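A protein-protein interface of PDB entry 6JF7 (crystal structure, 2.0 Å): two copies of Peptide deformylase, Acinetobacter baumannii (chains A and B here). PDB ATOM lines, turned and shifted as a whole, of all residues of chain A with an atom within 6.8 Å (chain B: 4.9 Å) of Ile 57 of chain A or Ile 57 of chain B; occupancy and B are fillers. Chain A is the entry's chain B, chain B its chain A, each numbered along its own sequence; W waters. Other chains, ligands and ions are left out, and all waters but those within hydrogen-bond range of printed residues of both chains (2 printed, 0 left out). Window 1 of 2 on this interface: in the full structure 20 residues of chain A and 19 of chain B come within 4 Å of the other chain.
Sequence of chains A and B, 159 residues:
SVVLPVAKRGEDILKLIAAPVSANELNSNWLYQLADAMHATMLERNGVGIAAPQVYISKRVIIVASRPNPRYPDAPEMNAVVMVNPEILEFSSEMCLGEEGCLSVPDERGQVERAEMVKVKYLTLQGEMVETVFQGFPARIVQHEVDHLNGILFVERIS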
ATOM      1  N   LEU A   4     -22.411   5.859 -16.395  1.00  0.00           N
ATOM      2  CA  LEU A   4     -21.593   4.822 -16.950  1.00  0.00           C
ATOM      3  C   LEU A   4     -21.557   4.919 -18.472  1.00  0.00           C
ATOM      4  O   LEU A   4     -22.482   5.433 -19.073  1.00  0.00           O
ATOM      5  CB  LEU A   4     -22.125   3.433 -16.593  1.00  0.00           C
ATOM      6  CG  LEU A   4     -22.174   2.976 -15.126  1.00  0.00           C
ATOM      7  CD1 LEU A   4     -22.959   1.667 -14.980  1.00  0.00           C
ATOM      8  CD2 LEU A   4     -20.753   2.785 -14.618  1.00  0.00           C
ATOM      9  N   ILE A  13     -21.085  -7.280 -26.801  1.00  0.00           N
ATOM     10  CA  ILE A  13     -21.688  -7.430 -25.455  1.00  0.00           C
ATOM     11  C   ILE A  13     -23.201  -7.418 -25.548  1.00  0.00           C
ATOM     12  O   ILE A  13     -23.883  -8.158 -24.857  1.00  0.00           O
ATOM     13  CB  ILE A  13     -21.181  -6.319 -24.506  1.00  0.00           C
ATOM     14  CG1 ILE A  13     -21.660  -6.483 -23.055  1.00  0.00           C
ATOM     15  CG2 ILE A  13     -21.595  -4.922 -24.953  1.00  0.00           C
ATOM     16  CD1 ILE A  13     -21.168  -7.682 -22.368  1.00  0.00           C
ATOM     17  N   ALA A  18     -27.497 -12.534 -21.275  1.00  0.00           N
ATOM     18  CA  ALA A  18     -26.951 -12.122 -19.980  1.00  0.00           C
ATOM     19  C   ALA A  18     -27.206 -13.209 -18.943  1.00  0.00           C
ATOM     20  O   ALA A  18     -28.247 -13.896 -18.987  1.00  0.00           O
ATOM     21  CB  ALA A  18     -27.590 -10.850 -19.543  1.00  0.00           C
ATOM     22  N   TRP A  30     -23.150  -4.698  -3.672  1.00  0.00           N
ATOM     23  CA  TRP A  30     -22.813  -4.866  -5.096  1.00  0.00           C
ATOM     24  C   TRP A  30     -24.050  -4.627  -6.027  1.00  0.00           C
ATOM     25  O   TRP A  30     -24.018  -3.762  -6.893  1.00  0.00           O
ATOM     26  CB  TRP A  30     -22.139  -6.239  -5.318  1.00  0.00           C
ATOM     27  CG  TRP A  30     -22.380  -6.856  -6.646  1.00  0.00           C
ATOM     28  CD1 TRP A  30     -23.189  -7.910  -6.930  1.00  0.00           C
ATOM     29  CD2 TRP A  30     -21.842  -6.418  -7.870  1.00  0.00           C
ATOM     30  NE1 TRP A  30     -23.174  -8.179  -8.267  1.00  0.00           N
ATOM     31  CE2 TRP A  30     -22.351  -7.283  -8.878  1.00  0.00           C
ATOM     32  CE3 TRP A  30     -20.934  -5.404  -8.219  1.00  0.00           C
ATOM     33  CZ2 TRP A  30     -21.994  -7.173 -10.205  1.00  0.00           C
ATOM     34  CZ3 TRP A  30     -20.617  -5.245  -9.529  1.00  0.00           C
ATOM     35  CH2 TRP A  30     -21.147  -6.136 -10.533  1.00  0.00           C
ATOM     36  N   LEU A  34     -24.858  -1.373  -8.493  1.00  0.00           N
ATOM     37  CA  LEU A  34     -25.085  -1.617  -9.937  1.00  0.00           C
ATOM     38  C   LEU A  34     -26.377  -0.939 -10.367  1.00  0.00           C
ATOM     39  O   LEU A  34     -26.410  -0.231 -11.365  1.00  0.00           O
ATOM     40  CB  LEU A  34     -25.187  -3.120 -10.244  1.00  0.00           C
ATOM     41  CG  LEU A  34     -25.747  -3.487 -11.644  1.00  0.00           C
ATOM     42  CD1 LEU A  34     -24.864  -2.896 -12.739  1.00  0.00           C
ATOM     43  CD2 LEU A  34     -25.799  -4.954 -11.849  1.00  0.00           C
ATOM     44  N   MET A  38     -26.847   2.179 -13.054  1.00  0.00           N
ATOM     45  CA  MET A  38     -27.801   2.056 -14.183  1.00  0.00           C
ATOM     46  C   MET A  38     -28.861   3.130 -14.207  1.00  0.00           C
ATOM     47  O   MET A  38     -29.117   3.732 -15.230  1.00  0.00           O
ATOM     48  CB  MET A  38     -28.471   0.677 -14.205  1.00  0.00           C
ATOM     49  CG  MET A  38     -27.496  -0.446 -14.533  1.00  0.00           C
ATOM     50  SD  MET A  38     -28.272  -2.072 -14.277  1.00  0.00           S
ATOM     51  CE  MET A  38     -29.610  -1.924 -15.500  1.00  0.00           C
ATOM     52  N   ALA A  51     -30.986  -1.660 -19.609  1.00  0.00           N
ATOM     53  CA  ALA A  51     -30.556  -3.038 -19.309  1.00  0.00           C
ATOM     54  C   ALA A  51     -29.054  -3.113 -19.034  1.00  0.00           C
ATOM     55  O   ALA A  51     -28.226  -2.430 -19.650  1.00  0.00           O
ATOM     56  CB  ALA A  51     -30.942  -3.967 -20.426  1.00  0.00           C
ATOM     57  N   ALA A  52     -28.684  -3.973 -18.091  1.00  0.00           N
ATOM     58  CA  ALA A  52     -27.279  -4.048 -17.670  1.00  0.00           C
ATOM     59  C   ALA A  52     -26.275  -4.226 -18.802  1.00  0.00           C
ATOM     60  O   ALA A  52     -25.195  -3.592 -18.807  1.00  0.00           O
ATOM     61  CB  ALA A  52     -27.079  -5.091 -16.620  1.00  0.00           C
ATOM     62  N   PRO A  53     -26.626  -5.071 -19.772  1.00  0.00           N
ATOM     63  CA  PRO A  53     -25.684  -5.224 -20.875  1.00  0.00           C
ATOM     64  C   PRO A  53     -25.298  -3.934 -21.611  1.00  0.00           C
ATOM     65  O   PRO A  53     -24.185  -3.852 -22.145  1.00  0.00           O
ATOM     66  CB  PRO A  53     -26.397  -6.168 -21.802  1.00  0.00           C
ATOM     67  CG  PRO A  53     -27.306  -6.962 -20.936  1.00  0.00           C
ATOM     68  CD  PRO A  53     -27.791  -5.951 -19.945  1.00  0.00           C
ATOM     69  N   GLN A  54     -26.208  -2.966 -21.614  1.00  0.00           N
ATOM     70  CA  GLN A  54     -25.969  -1.695 -22.239  1.00  0.00           C
ATOM     71  C   GLN A  54     -24.915  -0.889 -21.521  1.00  0.00           C
ATOM     72  O   GLN A  54     -24.312  -0.057 -22.139  1.00  0.00           O
ATOM     73  CB  GLN A  54     -27.242  -0.895 -22.371  1.00  0.00           C
ATOM     74  CG  GLN A  54     -28.299  -1.487 -23.261  1.00  0.00           C
ATOM     75  CD  GLN A  54     -29.485  -0.609 -23.271  1.00  0.00           C
ATOM     76  OE1 GLN A  54     -30.297  -0.613 -22.297  1.00  0.00           O
ATOM     77  NE2 GLN A  54     -29.562   0.256 -24.307  1.00  0.00           N
ATOM     78  N   VAL A  55     -24.606  -1.249 -20.279  1.00  0.00           N
ATOM     79  CA  VAL A  55     -23.474  -0.732 -19.565  1.00  0.00           C
ATOM     80  C   VAL A  55     -22.394  -1.733 -19.371  1.00  0.00           C
ATOM     81  O   VAL A  55     -21.605  -1.610 -18.433  1.00  0.00           O
ATOM     82  CB  VAL A  55     -23.896  -0.062 -18.233  1.00  0.00           C
ATOM     83  CG1 VAL A  55     -24.757   1.128 -18.523  1.00  0.00           C
ATOM     84  CG2 VAL A  55     -24.668  -1.015 -17.352  1.00  0.00           C
ATOM     85  N   TYR A  56     -22.274  -2.672 -20.322  1.00  0.00           N
ATOM     86  CA  TYR A  56     -21.202  -3.679 -20.303  1.00  0.00           C
ATOM     87  C   TYR A  56     -21.291  -4.696 -19.174  1.00  0.00           C
ATOM     88  O   TYR A  56     -20.288  -5.337 -18.808  1.00  0.00           O
ATOM     89  CB  TYR A  56     -19.808  -3.022 -20.319  1.00  0.00           C
ATOM     90  CG  TYR A  56     -19.563  -2.169 -21.532  1.00  0.00           C
ATOM     91  CD1 TYR A  56     -19.190  -2.755 -22.757  1.00  0.00           C
ATOM     92  CD2 TYR A  56     -19.710  -0.793 -21.484  1.00  0.00           C
ATOM     93  CE1 TYR A  56     -18.966  -1.996 -23.902  1.00  0.00           C
ATOM     94  CE2 TYR A  56     -19.502  -0.014 -22.628  1.00  0.00           C
ATOM     95  CZ  TYR A  56     -19.127  -0.627 -23.830  1.00  0.00           C
ATOM     96  OH  TYR A  56     -18.918   0.165 -24.932  1.00  0.00           O
ATOM     97  N   ILE A  57     -22.474  -4.900 -18.630  1.00  0.00           N
ATOM     98  CA  ILE A  57     -22.622  -5.816 -17.474  1.00  0.00           C
ATOM     99  C   ILE A  57     -23.587  -6.881 -17.912  1.00  0.00           C
ATOM    100  O   ILE A  57     -24.770  -6.626 -18.117  1.00  0.00           O
ATOM    101  CB  ILE A  57     -23.185  -5.124 -16.265  1.00  0.00           C
ATOM    102  CG1 ILE A  57     -22.346  -3.910 -15.913  1.00  0.00           C
ATOM    103  CG2 ILE A  57     -23.374  -6.127 -15.081  1.00  0.00           C
ATOM    104  CD1 ILE A  57     -21.055  -4.179 -15.225  1.00  0.00           C
ATOM    105  N   SER A  58     -23.096  -8.094 -18.049  1.00  0.00           N
ATOM    106  CA  SER A  58     -23.846  -9.150 -18.731  1.00  0.00           C
ATOM    107  C   SER A  58     -24.624  -9.904 -17.687  1.00  0.00           C
ATOM    108  O   SER A  58     -24.384 -11.101 -17.485  1.00  0.00           O
ATOM    109  CB  SER A  58     -22.940 -10.098 -19.570  1.00  0.00           C
ATOM    110  OG  SER A  58     -23.719 -10.844 -20.520  1.00  0.00           O
ATOM    111  N   LYS A  59     -25.541  -9.181 -17.027  1.00  0.00           N
ATOM    112  CA  LYS A  59     -26.333  -9.685 -15.935  1.00  0.00           C
ATOM    113  C   LYS A  59     -27.814  -9.331 -16.168  1.00  0.00           C
ATOM    114  O   LYS A  59     -28.133  -8.329 -16.788  1.00  0.00           O
ATOM    115  CB  LYS A  59     -25.858  -9.093 -14.634  1.00  0.00           C
ATOM    116  CG  LYS A  59     -24.488  -9.567 -14.208  1.00  0.00           C
ATOM    117  CD  LYS A  59     -24.589 -10.971 -13.579  1.00  0.00           C
ATOM    118  CE  LYS A  59     -23.571 -11.184 -12.476  1.00  0.00           C
ATOM    119  NZ  LYS A  59     -23.787 -12.556 -11.975  1.00  0.00           N
ATOM    120  N   ARG A  60     -28.722 -10.155 -15.663  1.00  0.00           N
ATOM    121  CA  ARG A  60     -30.124  -9.947 -15.934  1.00  0.00           C
ATOM    122  C   ARG A  60     -30.771  -8.917 -14.942  1.00  0.00           C
ATOM    123  O   ARG A  60     -31.507  -9.289 -14.012  1.00  0.00           O
ATOM    124  CB  ARG A  60     -30.815 -11.297 -15.972  1.00  0.00           C
ATOM    125  CG  ARG A  60     -30.233 -12.255 -17.011  1.00  0.00           C
ATOM    126  CD  ARG A  60     -30.955 -13.598 -17.108  1.00  0.00           C
ATOM    127  NE  ARG A  60     -32.076 -13.447 -17.966  1.00  0.00           N
ATOM    128  CZ  ARG A  60     -32.051 -13.431 -19.318  1.00  0.00           C
ATOM    129  NH1 ARG A  60     -30.924 -13.539 -20.026  1.00  0.00           N
ATOM    130  NH2 ARG A  60     -33.164 -13.183 -19.959  1.00  0.00           N
ATOM    131  N   VAL A  61     -30.451  -7.637 -15.149  1.00  0.00           N
ATOM    132  CA  VAL A  61     -31.010  -6.530 -14.366  1.00  0.00           C
ATOM    133  C   VAL A  61     -31.484  -5.480 -15.368  1.00  0.00           C
ATOM    134  O   VAL A  61     -30.735  -5.106 -16.245  1.00  0.00           O
ATOM    135  CB  VAL A  61     -30.027  -5.895 -13.415  1.00  0.00           C
ATOM    136  CG1 VAL A  61     -30.760  -4.822 -12.555  1.00  0.00           C
ATOM    137  CG2 VAL A  61     -29.433  -6.978 -12.501  1.00  0.00           C
ATOM    138  N   LEU A 149     -31.506  -8.383 -22.662  1.00  0.00           N
ATOM    139  CA  LEU A 149     -30.916  -9.462 -21.831  1.00  0.00           C
ATOM    140  C   LEU A 149     -30.736 -10.740 -22.617  1.00  0.00           C
ATOM    141  O   LEU A 149     -29.917 -11.584 -22.244  1.00  0.00           O
ATOM    142  CB  LEU A 149     -31.800  -9.783 -20.655  1.00  0.00           C
ATOM    143  CG  LEU A 149     -32.102  -8.688 -19.644  1.00  0.00           C
ATOM    144  CD1 LEU A 149     -32.801  -9.294 -18.451  1.00  0.00           C
ATOM    145  CD2 LEU A 149     -30.836  -7.998 -19.182  1.00  0.00           C
ATOM    146  N   TRP B  30     -19.259   2.438  -6.697  1.00  0.00           N
ATOM    147  CA  TRP B  30     -19.453   1.403  -7.729  1.00  0.00           C
ATOM    148  C   TRP B  30     -18.178   0.601  -7.998  1.00  0.00           C
ATOM    149  O   TRP B  30     -18.165  -0.621  -7.872  1.00  0.00           O
ATOM    150  CB  TRP B  30     -20.017   2.051  -9.007  1.00  0.00           C
ATOM    151  CG  TRP B  30     -19.692   1.385 -10.241  1.00  0.00           C
ATOM    152  CD1 TRP B  30     -18.888   1.867 -11.247  1.00  0.00           C
ATOM    153  CD2 TRP B  30     -20.129   0.101 -10.653  1.00  0.00           C
ATOM    154  NE1 TRP B  30     -18.796   0.954 -12.246  1.00  0.00           N
ATOM    155  CE2 TRP B  30     -19.555  -0.137 -11.929  1.00  0.00           C
ATOM    156  CE3 TRP B  30     -20.951  -0.887 -10.067  1.00  0.00           C
ATOM    157  CZ2 TRP B  30     -19.736  -1.323 -12.617  1.00  0.00           C
ATOM    158  CZ3 TRP B  30     -21.130  -2.084 -10.751  1.00  0.00           C
ATOM    159  CH2 TRP B  30     -20.518  -2.293 -12.023  1.00  0.00           C
ATOM    160  N   LEU B  34     -17.188  -3.265  -7.119  1.00  0.00           N
ATOM    161  CA  LEU B  34     -16.756  -4.232  -8.116  1.00  0.00           C
ATOM    162  C   LEU B  34     -15.423  -4.898  -7.731  1.00  0.00           C
ATOM    163  O   LEU B  34     -15.295  -6.102  -7.798  1.00  0.00           O
ATOM    164  CB  LEU B  34     -16.618  -3.585  -9.502  1.00  0.00           C
ATOM    165  CG  LEU B  34     -15.796  -4.425 -10.507  1.00  0.00           C
ATOM    166  CD1 LEU B  34     -16.555  -5.705 -10.843  1.00  0.00           C
ATOM    167  CD2 LEU B  34     -15.484  -3.677 -11.790  1.00  0.00           C
ATOM    168  N   ALA B  52     -12.249  -8.960 -14.790  1.00  0.00           N
ATOM    169  CA  ALA B  52     -13.692  -8.683 -14.705  1.00  0.00           C
ATOM    170  C   ALA B  52     -14.565  -9.488 -15.651  1.00  0.00           C
ATOM    171  O   ALA B  52     -15.639  -9.965 -15.253  1.00  0.00           O
ATOM    172  CB  ALA B  52     -13.940  -7.192 -14.840  1.00  0.00           C
ATOM    173  N   PRO B  53     -14.116  -9.699 -16.896  1.00  0.00           N
ATOM    174  CA  PRO B  53     -14.903 -10.577 -17.805  1.00  0.00           C
ATOM    175  C   PRO B  53     -15.304 -11.951 -17.255  1.00  0.00           C
ATOM    176  O   PRO B  53     -16.391 -12.494 -17.605  1.00  0.00           O
ATOM    177  CB  PRO B  53     -13.996 -10.685 -19.047  1.00  0.00           C
ATOM    178  CG  PRO B  53     -13.260  -9.374 -19.065  1.00  0.00           C
ATOM    179  CD  PRO B  53     -12.971  -9.084 -17.597  1.00  0.00           C
ATOM    180  N   VAL B  55     -16.245 -12.502 -14.318  1.00  0.00           N
ATOM    181  CA  VAL B  55     -17.433 -12.401 -13.477  1.00  0.00           C
ATOM    182  C   VAL B  55     -18.600 -11.677 -14.196  1.00  0.00           C
ATOM    183  O   VAL B  55     -19.422 -11.018 -13.570  1.00  0.00           O
ATOM    184  CB  VAL B  55     -17.109 -11.818 -12.072  1.00  0.00           C
ATOM    185  CG1 VAL B  55     -16.264 -12.817 -11.306  1.00  0.00           C
ATOM    186  CG2 VAL B  55     -16.426 -10.469 -12.187  1.00  0.00           C
ATOM    187  N   TYR B  56     -18.618 -11.811 -15.523  1.00  0.00           N
ATOM    188  CA  TYR B  56     -19.629 -11.227 -16.404  1.00  0.00           C
ATOM    189  C   TYR B  56     -19.616  -9.704 -16.519  1.00  0.00           C
ATOM    190  O   TYR B  56     -20.575  -9.113 -16.959  1.00  0.00           O
ATOM    191  CB  TYR B  56     -21.037 -11.771 -16.097  1.00  0.00           C
ATOM    192  CG  TYR B  56     -21.175 -13.252 -16.267  1.00  0.00           C
ATOM    193  CD1 TYR B  56     -21.483 -13.792 -17.514  1.00  0.00           C
ATOM    194  CD2 TYR B  56     -20.963 -14.141 -15.187  1.00  0.00           C
ATOM    195  CE1 TYR B  56     -21.613 -15.156 -17.671  1.00  0.00           C
ATOM    196  CE2 TYR B  56     -21.048 -15.524 -15.359  1.00  0.00           C
ATOM    197  CZ  TYR B  56     -21.377 -15.997 -16.589  1.00  0.00           C
ATOM    198  OH  TYR B  56     -21.488 -17.335 -16.794  1.00  0.00           O
ATOM    199  N   ILE B  57     -18.533  -9.068 -16.139  1.00  0.00           N
ATOM    200  CA  ILE B  57     -18.360  -7.595 -16.231  1.00  0.00           C
ATOM    201  C   ILE B  57     -17.338  -7.338 -17.362  1.00  0.00           C
ATOM    202  O   ILE B  57     -16.122  -7.575 -17.190  1.00  0.00           O
ATOM    203  CB  ILE B  57     -17.781  -7.065 -14.891  1.00  0.00           C
ATOM    204  CG1 ILE B  57     -18.577  -7.547 -13.673  1.00  0.00           C
ATOM    205  CG2 ILE B  57     -17.586  -5.543 -14.863  1.00  0.00           C
ATOM    206  CD1 ILE B  57     -20.041  -7.278 -13.763  1.00  0.00           C
ATOM    207  N   SER B  58     -17.792  -6.800 -18.489  1.00  0.00           N
ATOM    208  CA  SER B  58     -16.922  -6.593 -19.654  1.00  0.00           C
ATOM    209  C   SER B  58     -16.205  -5.221 -19.572  1.00  0.00           C
ATOM    210  O   SER B  58     -16.404  -4.311 -20.381  1.00  0.00           O
ATOM    211  CB  SER B  58     -17.714  -6.780 -20.944  1.00  0.00           C
ATOM    212  OG  SER B  58     -16.854  -7.050 -22.034  1.00  0.00           O
ATOM    213  N   LYS B  59     -15.343  -5.123 -18.569  1.00  0.00           N
ATOM    214  CA  LYS B  59     -14.622  -3.911 -18.234  1.00  0.00           C
ATOM    215  C   LYS B  59     -13.174  -4.284 -17.955  1.00  0.00           C
ATOM    216  O   LYS B  59     -12.887  -5.420 -17.541  1.00  0.00           O
ATOM    217  CB  LYS B  59     -15.285  -3.211 -17.043  1.00  0.00           C
ATOM    218  CG  LYS B  59     -16.654  -2.665 -17.381  1.00  0.00           C
ATOM    219  CD  LYS B  59     -17.078  -1.617 -16.350  1.00  0.00           C
ATOM    220  CE  LYS B  59     -18.172  -0.670 -16.865  1.00  0.00           C
ATOM    221  NZ  LYS B  59     -17.652   0.574 -17.508  1.00  0.00           N
HETATM  222  O   HOH W   1     -20.720 -12.827 -11.994  1.00  0.00           O
HETATM  223  O   HOH W   2     -20.449   0.797 -18.408  1.00  0.00           O
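The backbone carbonyl oxygen of Ala 52 of chain A sits at hydrogen-bond distance from the backbone NH of Ile 57 of chain A, 3.0 Å away.
The backbone carbonyl oxygen (O) of Ala 52 of chain B sits at hydrogen-bond distance from the backbone NH (N) of Ile 57 of chain B (3.2 Å).
Printed residues of chain B within 4 Å of Leu 4 of chain A: Trp 30 (3.6 Å).
Of the printed residues of chain B, Trp 30 of chain A touches Trp 30 and Ile 57.
Gln 54 of chain A touches none of the printed residues of chain B.
Of the printed residues of chain B, Val 55 of chain A touches Lys 59.
Of the printed residues of chain B, Tyr 56 of chain A touches Ile 57 (3.8 Å) and Ser 58 (2.9 Å).
Pro 53 of chain B touches none of the printed residues of chain A.
Ile 57 of chain B touches just these residues of chain A: Trp 30 (3.6 Å), Tyr 56 (3.8 Å) and Ile 57 (3.6 Å).
The nearest residue of chain B that does not touch Ile 57 of chain A is Lys 59 of chain B (4.8 Å).
The nearest printed residue of chain A that does not touch Ile 57 of chain B is Lys 59 of chain A (5.0 Å).
NE1 of Trp 30 of chain B touches CD2 of Leu 4 of chain A, 3.6 Å away.
Ile 13 of chain A touches Ser 58 of chain B (CD1 to CB, 3.8 Å).
Trp 30 of chain A touches Trp 30 of chain B.
Ile 57 of chain B touches Trp 30 of chain A.
O of Val 55 of chain A touches CE of Lys 59 of chain B (3.9 Å).
Tyr 56 of chain A touches Ile 57 of chain B.
Ile 57 of chain A touches Trp 30 of chain B (CD1 to CH2, 3.8 Å).
Ile 57 of chain A touches Tyr 56 of chain B (C to O, 3.9 Å).
CD1 of Ile 57 of chain A touches CD1 of Ile 57 of chain B, at 3.6 Å.
O of Tyr 56 of chain B is in hydrogen-bond range of N of Ser 58 of chain A.
N of Ser 58 of chain B sits at hydrogen-bond distance from O of Tyr 56 of chain A, at 2.9 Å.
Water W2 lies within hydrogen-bond range of O of Val 55 of chain A (2.7 Å) and NZ of Lys 59 of chain B (2.9 Å).
Water W1 bridges O of Val 55 of chain B and NZ of Lys 59 of chain A.
Of the 9 printed residues of chain B, 5 touch a printed residue of chain A.
Printed residues of chain B that touch a printed residue of chain A: Trp 30, Tyr 56, Ile 57, Ser 58 and Lys 59.
Hydrophobic or aromatic side chains of chain B within 4 Å of the printed part of chain A: Trp 30, Tyr 56 and Ile 57.
Along chain A the printed residues that touch a printed residue of chain B span positions 4 to 58.
Among the printed residues, no Asp or Glu carboxylate lies within 4 Å of a Lys or Arg side-chain nitrogen of the other chain.
Trp 30 of chain B touches its own counterpart, Trp 30 of chain A.
Trp 30 of chain A touches Ile 57 of chain B, and with the chains exchanged Ile 57 of chain A touches Trp 30 of chain B.
Tyr 56 of chain A touches Ser 58 of chain B, and with the chains exchanged Ser 58 of chain A touches Tyr 56 of chain B.
Ile 57 of chain A touches its own counterpart, Ile 57 of chain B.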
